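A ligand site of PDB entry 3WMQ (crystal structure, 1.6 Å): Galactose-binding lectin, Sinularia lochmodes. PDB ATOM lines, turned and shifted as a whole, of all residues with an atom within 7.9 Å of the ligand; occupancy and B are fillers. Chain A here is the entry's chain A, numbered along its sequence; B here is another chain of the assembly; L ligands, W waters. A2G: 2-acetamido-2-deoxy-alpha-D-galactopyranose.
Water W3 bridges an oxygen (O7) of the ligand and the backbone NH (N) of Tyr 79. Water W1 bridges an oxygen (O3) of the ligand (2.8 Å) and the side-chain amide nitrogen of Asn 85 of chain B (3.0 Å).
The side-chain hydroxyl of Thr 81 sits close to the backbone carbonyl oxygen of Trp 78 (3.5 Å). NH2 of Arg 58 lies close to ND2 of Asn 56, at 3.5 Å. OG1 of Thr 81 lies within hydrogen-bond range of O of Asn 56 (2.7 Å). The guanidinium group (NH1) of Arg 58 is in hydrogen-bond range of the side-chain hydroxyl (OG1) of Thr 80, 3.0 Å away. The side-chain carboxylate of Asp 52 of chain B lies within hydrogen-bond range of the indole nitrogen of Trp 84 of chain B (2.9 Å). The guanidinium group of Arg 58 is in hydrogen-bond range of the side-chain hydroxyl of Thr 81 (3.0 Å). The backbone NH of Trp 18 of chain B sits at hydrogen-bond distance from the backbone carbonyl oxygen of Trp 84 of chain B, 2.9 Å away. OD1 of Asp 50 of chain B sits at hydrogen-bond distance from ND2 of Asn 85 of chain B.
An oxygen (O4) of the ligand is in hydrogen-bond range of the side-chain carboxylate of Asp 50 of chain B, 2.6 Å away. An oxygen (O5) of the ligand is in hydrogen-bond range of the guanidinium group (NH2) of Arg 58 (2.9 Å). The indole nitrogen (NE1) of Trp 78 sits at hydrogen-bond distance from an oxygen (O4) of the ligand (3.0 Å). The side-chain amide nitrogen of Asn 56 sits at hydrogen-bond distance from an oxygen (O6) of the ligand (2.9 Å).
Tyr 79 touches the ligand. CZ2 of Trp 18 of chain B touches O1 of the ligand, 3.1 Å away. CD1 of Trp 84 of chain B touches C6 of the ligand, 3.5 Å away. Hydrophobic or aromatic side chains that line the ligand: Trp 78, Tyr 79, Trp 18 of chain B and Trp 84 of chain B. Within 4 Å of the ligand: Asn 56, Arg 58, Trp 78, Tyr 79, Trp 18 of chain B, Asp 50 of chain B and Trp 84 of chain B. The nearest printed residue that does not touch the ligand is Asn 85 of chain B (4.4 Å).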
ATOM      1  N   ASN A  55      26.258  23.179 -16.259  1.00  0.00           N
ATOM      2  CA  ASN A  55      25.095  22.428 -16.725  1.00  0.00           C
ATOM      3  C   ASN A  55      23.852  23.301 -16.577  1.00  0.00           C
ATOM      4  O   ASN A  55      23.927  24.389 -15.999  1.00  0.00           O
ATOM      5  CB  ASN A  55      24.939  21.145 -15.902  1.00  0.00           C
ATOM      6  CG  ASN A  55      26.041  20.140 -16.195  1.00  0.00           C
ATOM      7  OD1 ASN A  55      26.047  19.496 -17.248  1.00  0.00           O
ATOM      8  ND2 ASN A  55      26.988  20.008 -15.266  1.00  0.00           N
ATOM      9  N   ASN A  56      22.723  22.845 -17.109  1.00  0.00           N
ATOM     10  CA  ASN A  56      21.486  23.606 -17.014  1.00  0.00           C
ATOM     11  C   ASN A  56      21.109  23.820 -15.560  1.00  0.00           C
ATOM     12  O   ASN A  56      21.523  23.071 -14.678  1.00  0.00           O
ATOM     13  CB  ASN A  56      20.330  22.875 -17.709  1.00  0.00           C
ATOM     14  CG  ASN A  56      20.499  22.776 -19.211  1.00  0.00           C
ATOM     15  OD1 ASN A  56      21.417  23.348 -19.800  1.00  0.00           O
ATOM     16  ND2 ASN A  56      19.578  22.052 -19.851  1.00  0.00           N
ATOM     17  N   LEU A  57      20.300  24.841 -15.302  1.00  0.00           N
ATOM     18  CA  LEU A  57      19.837  25.118 -13.961  1.00  0.00           C
ATOM     19  C   LEU A  57      18.496  24.416 -13.804  1.00  0.00           C
ATOM     20  O   LEU A  57      17.586  24.652 -14.582  1.00  0.00           O
ATOM     21  CB  LEU A  57      19.692  26.635 -13.740  1.00  0.00           C
ATOM     22  CG  LEU A  57      19.101  27.104 -12.399  1.00  0.00           C
ATOM     23  CD1 LEU A  57      19.702  28.452 -12.047  1.00  0.00           C
ATOM     24  CD2 LEU A  57      17.579  27.196 -12.483  1.00  0.00           C
ATOM     25  N   ARG A  58      18.426  23.513 -12.832  1.00  0.00           N
ATOM     26  CA  ARG A  58      17.195  22.765 -12.566  1.00  0.00           C
ATOM     27  C   ARG A  58      16.989  22.763 -11.052  1.00  0.00           C
ATOM     28  O   ARG A  58      17.723  22.076 -10.329  1.00  0.00           O
ATOM     29  CB  ARG A  58      17.322  21.313 -13.041  1.00  0.00           C
ATOM     30  CG  ARG A  58      17.668  21.137 -14.509  1.00  0.00           C
ATOM     31  CD  ARG A  58      17.876  19.659 -14.825  1.00  0.00           C
ATOM     32  NE  ARG A  58      18.285  19.425 -16.208  1.00  0.00           N
ATOM     33  CZ  ARG A  58      19.546  19.404 -16.639  1.00  0.00           C
ATOM     34  NH1 ARG A  58      20.544  19.592 -15.781  1.00  0.00           N
ATOM     35  NH2 ARG A  58      19.810  19.196 -17.918  1.00  0.00           N
ATOM     36  N   SER A  77      17.042  19.048  -7.041  1.00  0.00           N
ATOM     37  CA  SER A  77      17.531  19.458  -8.340  1.00  0.00           C
ATOM     38  C   SER A  77      17.415  18.141  -9.048  1.00  0.00           C
ATOM     39  O   SER A  77      16.931  17.181  -8.459  1.00  0.00           O
ATOM     40  CB  SER A  77      19.005  19.931  -8.268  1.00  0.00           C
ATOM     41  OG  SER A  77      19.846  18.949  -7.679  1.00  0.00           O
ATOM     42  N   TRP A  78      17.835  18.089 -10.310  1.00  0.00           N
ATOM     43  CA  TRP A  78      17.797  16.817 -11.023  1.00  0.00           C
ATOM     44  C   TRP A  78      18.809  16.818 -12.176  1.00  0.00           C
ATOM     45  O   TRP A  78      19.471  17.829 -12.436  1.00  0.00           O
ATOM     46  CB  TRP A  78      16.364  16.439 -11.484  1.00  0.00           C
ATOM     47  CG  TRP A  78      15.692  17.280 -12.537  1.00  0.00           C
ATOM     48  CD1 TRP A  78      15.571  16.980 -13.860  1.00  0.00           C
ATOM     49  CD2 TRP A  78      15.022  18.526 -12.333  1.00  0.00           C
ATOM     50  NE1 TRP A  78      14.862  17.968 -14.506  1.00  0.00           N
ATOM     51  CE2 TRP A  78      14.515  18.932 -13.594  1.00  0.00           C
ATOM     52  CE3 TRP A  78      14.805  19.343 -11.216  1.00  0.00           C
ATOM     53  CZ2 TRP A  78      13.807  20.127 -13.765  1.00  0.00           C
ATOM     54  CZ3 TRP A  78      14.088  20.532 -11.386  1.00  0.00           C
ATOM     55  CH2 TRP A  78      13.599  20.913 -12.654  1.00  0.00           C
ATOM     56  N   TYR A  79      18.955  15.666 -12.808  1.00  0.00           N
ATOM     57  CA  TYR A  79      19.922  15.440 -13.886  1.00  0.00           C
ATOM     58  C   TYR A  79      21.309  15.964 -13.497  1.00  0.00           C
ATOM     59  O   TYR A  79      21.749  15.758 -12.376  1.00  0.00           O
ATOM     60  CB  TYR A  79      19.447  16.038 -15.224  1.00  0.00           C
ATOM     61  CG  TYR A  79      20.015  15.251 -16.416  1.00  0.00           C
ATOM     62  CD1 TYR A  79      19.876  13.863 -16.485  1.00  0.00           C
ATOM     63  CD2 TYR A  79      20.693  15.903 -17.451  1.00  0.00           C
ATOM     64  CE1 TYR A  79      20.396  13.137 -17.580  1.00  0.00           C
ATOM     65  CE2 TYR A  79      21.209  15.187 -18.537  1.00  0.00           C
ATOM     66  CZ  TYR A  79      21.066  13.810 -18.587  1.00  0.00           C
ATOM     67  OH  TYR A  79      21.563  13.106 -19.663  1.00  0.00           O
ATOM     68  N   THR A  80      21.976  16.628 -14.431  1.00  0.00           N
ATOM     69  CA  THR A  80      23.348  17.124 -14.240  1.00  0.00           C
ATOM     70  C   THR A  80      23.567  18.413 -13.447  1.00  0.00           C
ATOM     71  O   THR A  80      24.701  18.864 -13.283  1.00  0.00           O
ATOM     72  CB  THR A  80      23.999  17.312 -15.590  1.00  0.00           C
ATOM     73  OG1 THR A  80      23.176  18.190 -16.367  1.00  0.00           O
ATOM     74  CG2 THR A  80      24.132  15.979 -16.311  1.00  0.00           C
ATOM     75  N   THR A  81      22.488  19.015 -12.964  1.00  0.00           N
ATOM     76  CA  THR A  81      22.581  20.267 -12.233  1.00  0.00           C
ATOM     77  C   THR A  81      23.405  20.176 -10.949  1.00  0.00           C
ATOM     78  O   THR A  81      23.313  19.198 -10.197  1.00  0.00           O
ATOM     79  CB  THR A  81      21.166  20.777 -11.911  1.00  0.00           C
ATOM     80  OG1 THR A  81      20.494  21.076 -13.135  1.00  0.00           O
ATOM     81  CG2 THR A  81      21.211  22.019 -11.040  1.00  0.00           C
ATOM     82  N   ARG B  16       5.137  22.048 -17.456  1.00  0.00           N
ATOM     83  CA  ARG B  16       6.086  20.990 -17.763  1.00  0.00           C
ATOM     84  C   ARG B  16       6.138  20.927 -19.279  1.00  0.00           C
ATOM     85  O   ARG B  16       5.204  20.444 -19.920  1.00  0.00           O
ATOM     86  CB  ARG B  16       5.611  19.645 -17.201  1.00  0.00           C
ATOM     87  CG  ARG B  16       5.749  19.511 -15.702  1.00  0.00           C
ATOM     88  CD  ARG B  16       5.734  18.059 -15.284  1.00  0.00           C
ATOM     89  NE  ARG B  16       6.339  17.843 -13.975  1.00  0.00           N
ATOM     90  CZ  ARG B  16       7.653  17.809 -13.746  1.00  0.00           C
ATOM     91  NH1 ARG B  16       8.517  17.977 -14.738  1.00  0.00           N
ATOM     92  NH2 ARG B  16       8.101  17.595 -12.512  1.00  0.00           N
ATOM     93  N   TRP B  18       9.428  20.191 -21.259  1.00  0.00           N
ATOM     94  CA  TRP B  18      10.372  19.188 -21.739  1.00  0.00           C
ATOM     95  C   TRP B  18       9.595  17.951 -22.173  1.00  0.00           C
ATOM     96  O   TRP B  18       8.721  17.500 -21.457  1.00  0.00           O
ATOM     97  CB  TRP B  18      11.335  18.835 -20.620  1.00  0.00           C
ATOM     98  CG  TRP B  18      12.275  17.750 -20.993  1.00  0.00           C
ATOM     99  CD1 TRP B  18      12.178  16.418 -20.658  1.00  0.00           C
ATOM    100  CD2 TRP B  18      13.442  17.875 -21.797  1.00  0.00           C
ATOM    101  NE1 TRP B  18      13.221  15.719 -21.223  1.00  0.00           N
ATOM    102  CE2 TRP B  18      14.010  16.584 -21.930  1.00  0.00           C
ATOM    103  CE3 TRP B  18      14.064  18.959 -22.432  1.00  0.00           C
ATOM    104  CZ2 TRP B  18      15.163  16.354 -22.660  1.00  0.00           C
ATOM    105  CZ3 TRP B  18      15.223  18.721 -23.161  1.00  0.00           C
ATOM    106  CH2 TRP B  18      15.764  17.424 -23.270  1.00  0.00           C
ATOM    107  N   PRO B  19       9.965  17.346 -23.323  1.00  0.00           N
ATOM    108  CA  PRO B  19      11.048  17.685 -24.247  1.00  0.00           C
ATOM    109  C   PRO B  19      10.872  18.825 -25.264  1.00  0.00           C
ATOM    110  O   PRO B  19      11.552  18.840 -26.280  1.00  0.00           O
ATOM    111  CB  PRO B  19      11.343  16.353 -24.915  1.00  0.00           C
ATOM    112  CG  PRO B  19      10.000  15.736 -25.037  1.00  0.00           C
ATOM    113  CD  PRO B  19       9.289  16.099 -23.736  1.00  0.00           C
ATOM    114  N   ARG B  20       9.982  19.775 -24.984  1.00  0.00           N
ATOM    115  CA  ARG B  20       9.835  20.938 -25.855  1.00  0.00           C
ATOM    116  C   ARG B  20      10.118  22.133 -24.982  1.00  0.00           C
ATOM    117  O   ARG B  20      10.022  22.023 -23.757  1.00  0.00           O
ATOM    118  CB  ARG B  20       8.400  21.090 -26.398  1.00  0.00           C
ATOM    119  CG  ARG B  20       8.012  20.078 -27.424  1.00  0.00           C
ATOM    120  CD  ARG B  20       6.739  20.515 -28.106  1.00  0.00           C
ATOM    121  NE  ARG B  20       6.301  19.510 -29.057  1.00  0.00           N
ATOM    122  CZ  ARG B  20       5.193  19.604 -29.778  1.00  0.00           C
ATOM    123  NH1 ARG B  20       4.408  20.667 -29.663  1.00  0.00           N
ATOM    124  NH2 ARG B  20       4.869  18.631 -30.624  1.00  0.00           N
ATOM    125  N   LEU B  49      12.276  25.802 -11.667  1.00  0.00           N
ATOM    126  CA  LEU B  49      12.809  26.402 -12.892  1.00  0.00           C
ATOM    127  C   LEU B  49      13.830  25.468 -13.525  1.00  0.00           C
ATOM    128  O   LEU B  49      14.646  24.865 -12.836  1.00  0.00           O
ATOM    129  CB  LEU B  49      13.451  27.754 -12.565  1.00  0.00           C
ATOM    130  CG  LEU B  49      13.873  28.625 -13.744  1.00  0.00           C
ATOM    131  CD1 LEU B  49      12.647  28.917 -14.619  1.00  0.00           C
ATOM    132  CD2 LEU B  49      14.467  29.934 -13.220  1.00  0.00           C
ATOM    133  N   ASP B  50      13.763  25.371 -14.849  1.00  0.00           N
ATOM    134  CA  ASP B  50      14.655  24.525 -15.647  1.00  0.00           C
ATOM    135  C   ASP B  50      15.055  25.404 -16.845  1.00  0.00           C
ATOM    136  O   ASP B  50      14.276  25.600 -17.773  1.00  0.00           O
ATOM    137  CB  ASP B  50      13.862  23.277 -16.077  1.00  0.00           C
ATOM    138  CG  ASP B  50      14.688  22.282 -16.872  1.00  0.00           C
ATOM    139  OD1 ASP B  50      14.191  21.140 -17.058  1.00  0.00           O
ATOM    140  OD2 ASP B  50      15.797  22.621 -17.319  1.00  0.00           O
ATOM    141  N   VAL B  51      16.274  25.948 -16.777  1.00  0.00           N
ATOM    142  CA  VAL B  51      16.793  26.857 -17.800  1.00  0.00           C
ATOM    143  C   VAL B  51      18.081  26.348 -18.445  1.00  0.00           C
ATOM    144  O   VAL B  51      19.005  25.925 -17.758  1.00  0.00           O
ATOM    145  CB  VAL B  51      17.056  28.240 -17.171  1.00  0.00           C
ATOM    146  CG1 VAL B  51      17.632  29.203 -18.209  1.00  0.00           C
ATOM    147  CG2 VAL B  51      15.753  28.793 -16.614  1.00  0.00           C
ATOM    148  N   ASP B  52      18.142  26.421 -19.771  1.00  0.00           N
ATOM    149  CA  ASP B  52      19.323  25.951 -20.483  1.00  0.00           C
ATOM    150  C   ASP B  52      20.526  26.871 -20.285  1.00  0.00           C
ATOM    151  O   ASP B  52      20.410  28.092 -20.373  1.00  0.00           O
ATOM    152  CB  ASP B  52      19.015  25.821 -21.968  1.00  0.00           C
ATOM    153  CG  ASP B  52      19.862  24.754 -22.630  1.00  0.00           C
ATOM    154  OD1 ASP B  52      21.067  24.987 -22.834  1.00  0.00           O
ATOM    155  OD2 ASP B  52      19.308  23.672 -22.922  1.00  0.00           O
ATOM    156  N   ASN B  53      21.680  26.268 -20.031  1.00  0.00           N
ATOM    157  CA  ASN B  53      22.890  27.044 -19.820  1.00  0.00           C
ATOM    158  C   ASN B  53      23.519  27.521 -21.126  1.00  0.00           C
ATOM    159  O   ASN B  53      24.534  28.209 -21.103  1.00  0.00           O
ATOM    160  CB  ASN B  53      23.911  26.256 -18.998  1.00  0.00           C
ATOM    161  CG  ASN B  53      24.525  25.091 -19.771  1.00  0.00           C
ATOM    162  OD1 ASN B  53      23.973  24.623 -20.773  1.00  0.00           O
ATOM    163  ND2 ASN B  53      25.671  24.591 -19.290  1.00  0.00           N
ATOM    164  N   THR B  82      16.301  29.834 -23.115  1.00  0.00           N
ATOM    165  CA  THR B  82      15.510  28.643 -23.361  1.00  0.00           C
ATOM    166  C   THR B  82      15.094  28.079 -22.012  1.00  0.00           C
ATOM    167  O   THR B  82      15.946  27.754 -21.171  1.00  0.00           O
ATOM    168  CB  THR B  82      16.320  27.574 -24.132  1.00  0.00           C
ATOM    169  OG1 THR B  82      16.610  28.059 -25.453  1.00  0.00           O
ATOM    170  CG2 THR B  82      15.545  26.271 -24.228  1.00  0.00           C
ATOM    171  N   VAL B  83      13.792  27.999 -21.804  1.00  0.00           N
ATOM    172  CA  VAL B  83      13.244  27.477 -20.560  1.00  0.00           C
ATOM    173  C   VAL B  83      12.523  26.168 -20.875  1.00  0.00           C
ATOM    174  O   VAL B  83      11.653  26.123 -21.762  1.00  0.00           O
ATOM    175  CB  VAL B  83      12.272  28.497 -19.937  1.00  0.00           C
ATOM    176  CG1 VAL B  83      11.731  27.976 -18.612  1.00  0.00           C
ATOM    177  CG2 VAL B  83      13.003  29.830 -19.719  1.00  0.00           C
ATOM    178  N   TRP B  84      12.890  25.118 -20.161  1.00  0.00           N
ATOM    179  CA  TRP B  84      12.331  23.778 -20.366  1.00  0.00           C
ATOM    180  C   TRP B  84      11.174  23.383 -19.445  1.00  0.00           C
ATOM    181  O   TRP B  84      10.363  22.518 -19.787  1.00  0.00           O
ATOM    182  CB  TRP B  84      13.443  22.745 -20.226  1.00  0.00           C
ATOM    183  CG  TRP B  84      14.526  22.860 -21.254  1.00  0.00           C
ATOM    184  CD1 TRP B  84      15.816  23.282 -21.051  1.00  0.00           C
ATOM    185  CD2 TRP B  84      14.435  22.502 -22.631  1.00  0.00           C
ATOM    186  NE1 TRP B  84      16.538  23.189 -22.227  1.00  0.00           N
ATOM    187  CE2 TRP B  84      15.713  22.706 -23.206  1.00  0.00           C
ATOM    188  CE3 TRP B  84      13.407  22.008 -23.443  1.00  0.00           C
ATOM    189  CZ2 TRP B  84      15.976  22.441 -24.557  1.00  0.00           C
ATOM    190  CZ3 TRP B  84      13.671  21.744 -24.784  1.00  0.00           C
ATOM    191  CH2 TRP B  84      14.947  21.962 -25.320  1.00  0.00           C
ATOM    192  N   ASN B  85      11.117  24.000 -18.270  1.00  0.00           N
ATOM    193  CA  ASN B  85      10.070  23.720 -17.279  1.00  0.00           C
ATOM    194  C   ASN B  85      10.075  24.869 -16.275  1.00  0.00           C
ATOM    195  O   ASN B  85      11.123  25.463 -16.035  1.00  0.00           O
ATOM    196  CB  ASN B  85      10.383  22.452 -16.449  1.00  0.00           C
ATOM    197  CG  ASN B  85      10.302  21.166 -17.237  1.00  0.00           C
ATOM    198  OD1 ASN B  85       9.221  20.741 -17.677  1.00  0.00           O
ATOM    199  ND2 ASN B  85      11.439  20.488 -17.387  1.00  0.00           N
HETATM  200  O5  A2G L   1      17.493  18.035 -19.146  1.00  0.00           O
HETATM  201  C1  A2G L   1      17.420  16.601 -19.020  1.00  0.00           C
HETATM  202  O1  A2G L   1      17.084  16.072 -20.259  1.00  0.00           O
HETATM  203  C2  A2G L   1      16.350  16.194 -17.984  1.00  0.00           C
HETATM  204  N2  A2G L   1      16.196  14.746 -18.031  1.00  0.00           N
HETATM  205  C3  A2G L   1      15.011  16.852 -18.319  1.00  0.00           C
HETATM  206  O3  A2G L   1      14.081  16.601 -17.275  1.00  0.00           O
HETATM  207  C4  A2G L   1      15.179  18.365 -18.489  1.00  0.00           C
HETATM  208  O4  A2G L   1      15.579  18.930 -17.243  1.00  0.00           O
HETATM  209  C5  A2G L   1      16.246  18.629 -19.551  1.00  0.00           C
HETATM  210  C6  A2G L   1      16.495  20.118 -19.828  1.00  0.00           C
HETATM  211  O6  A2G L   1      17.213  20.743 -18.760  1.00  0.00           O
HETATM  212  C7  A2G L   1      16.287  14.014 -16.923  1.00  0.00           C
HETATM  213  O7  A2G L   1      16.461  14.486 -15.800  1.00  0.00           O
HETATM  214  C8  A2G L   1      16.143  12.512 -17.095  1.00  0.00           C
HETATM  215  O   HOH W   1      11.386  17.445 -17.340  1.00  0.00           O
HETATM  216  O   HOH W   2      12.877  14.004 -17.578  1.00  0.00           O
HETATM  217  O   HOH W   3      16.946  13.469 -13.368  1.00  0.00           O
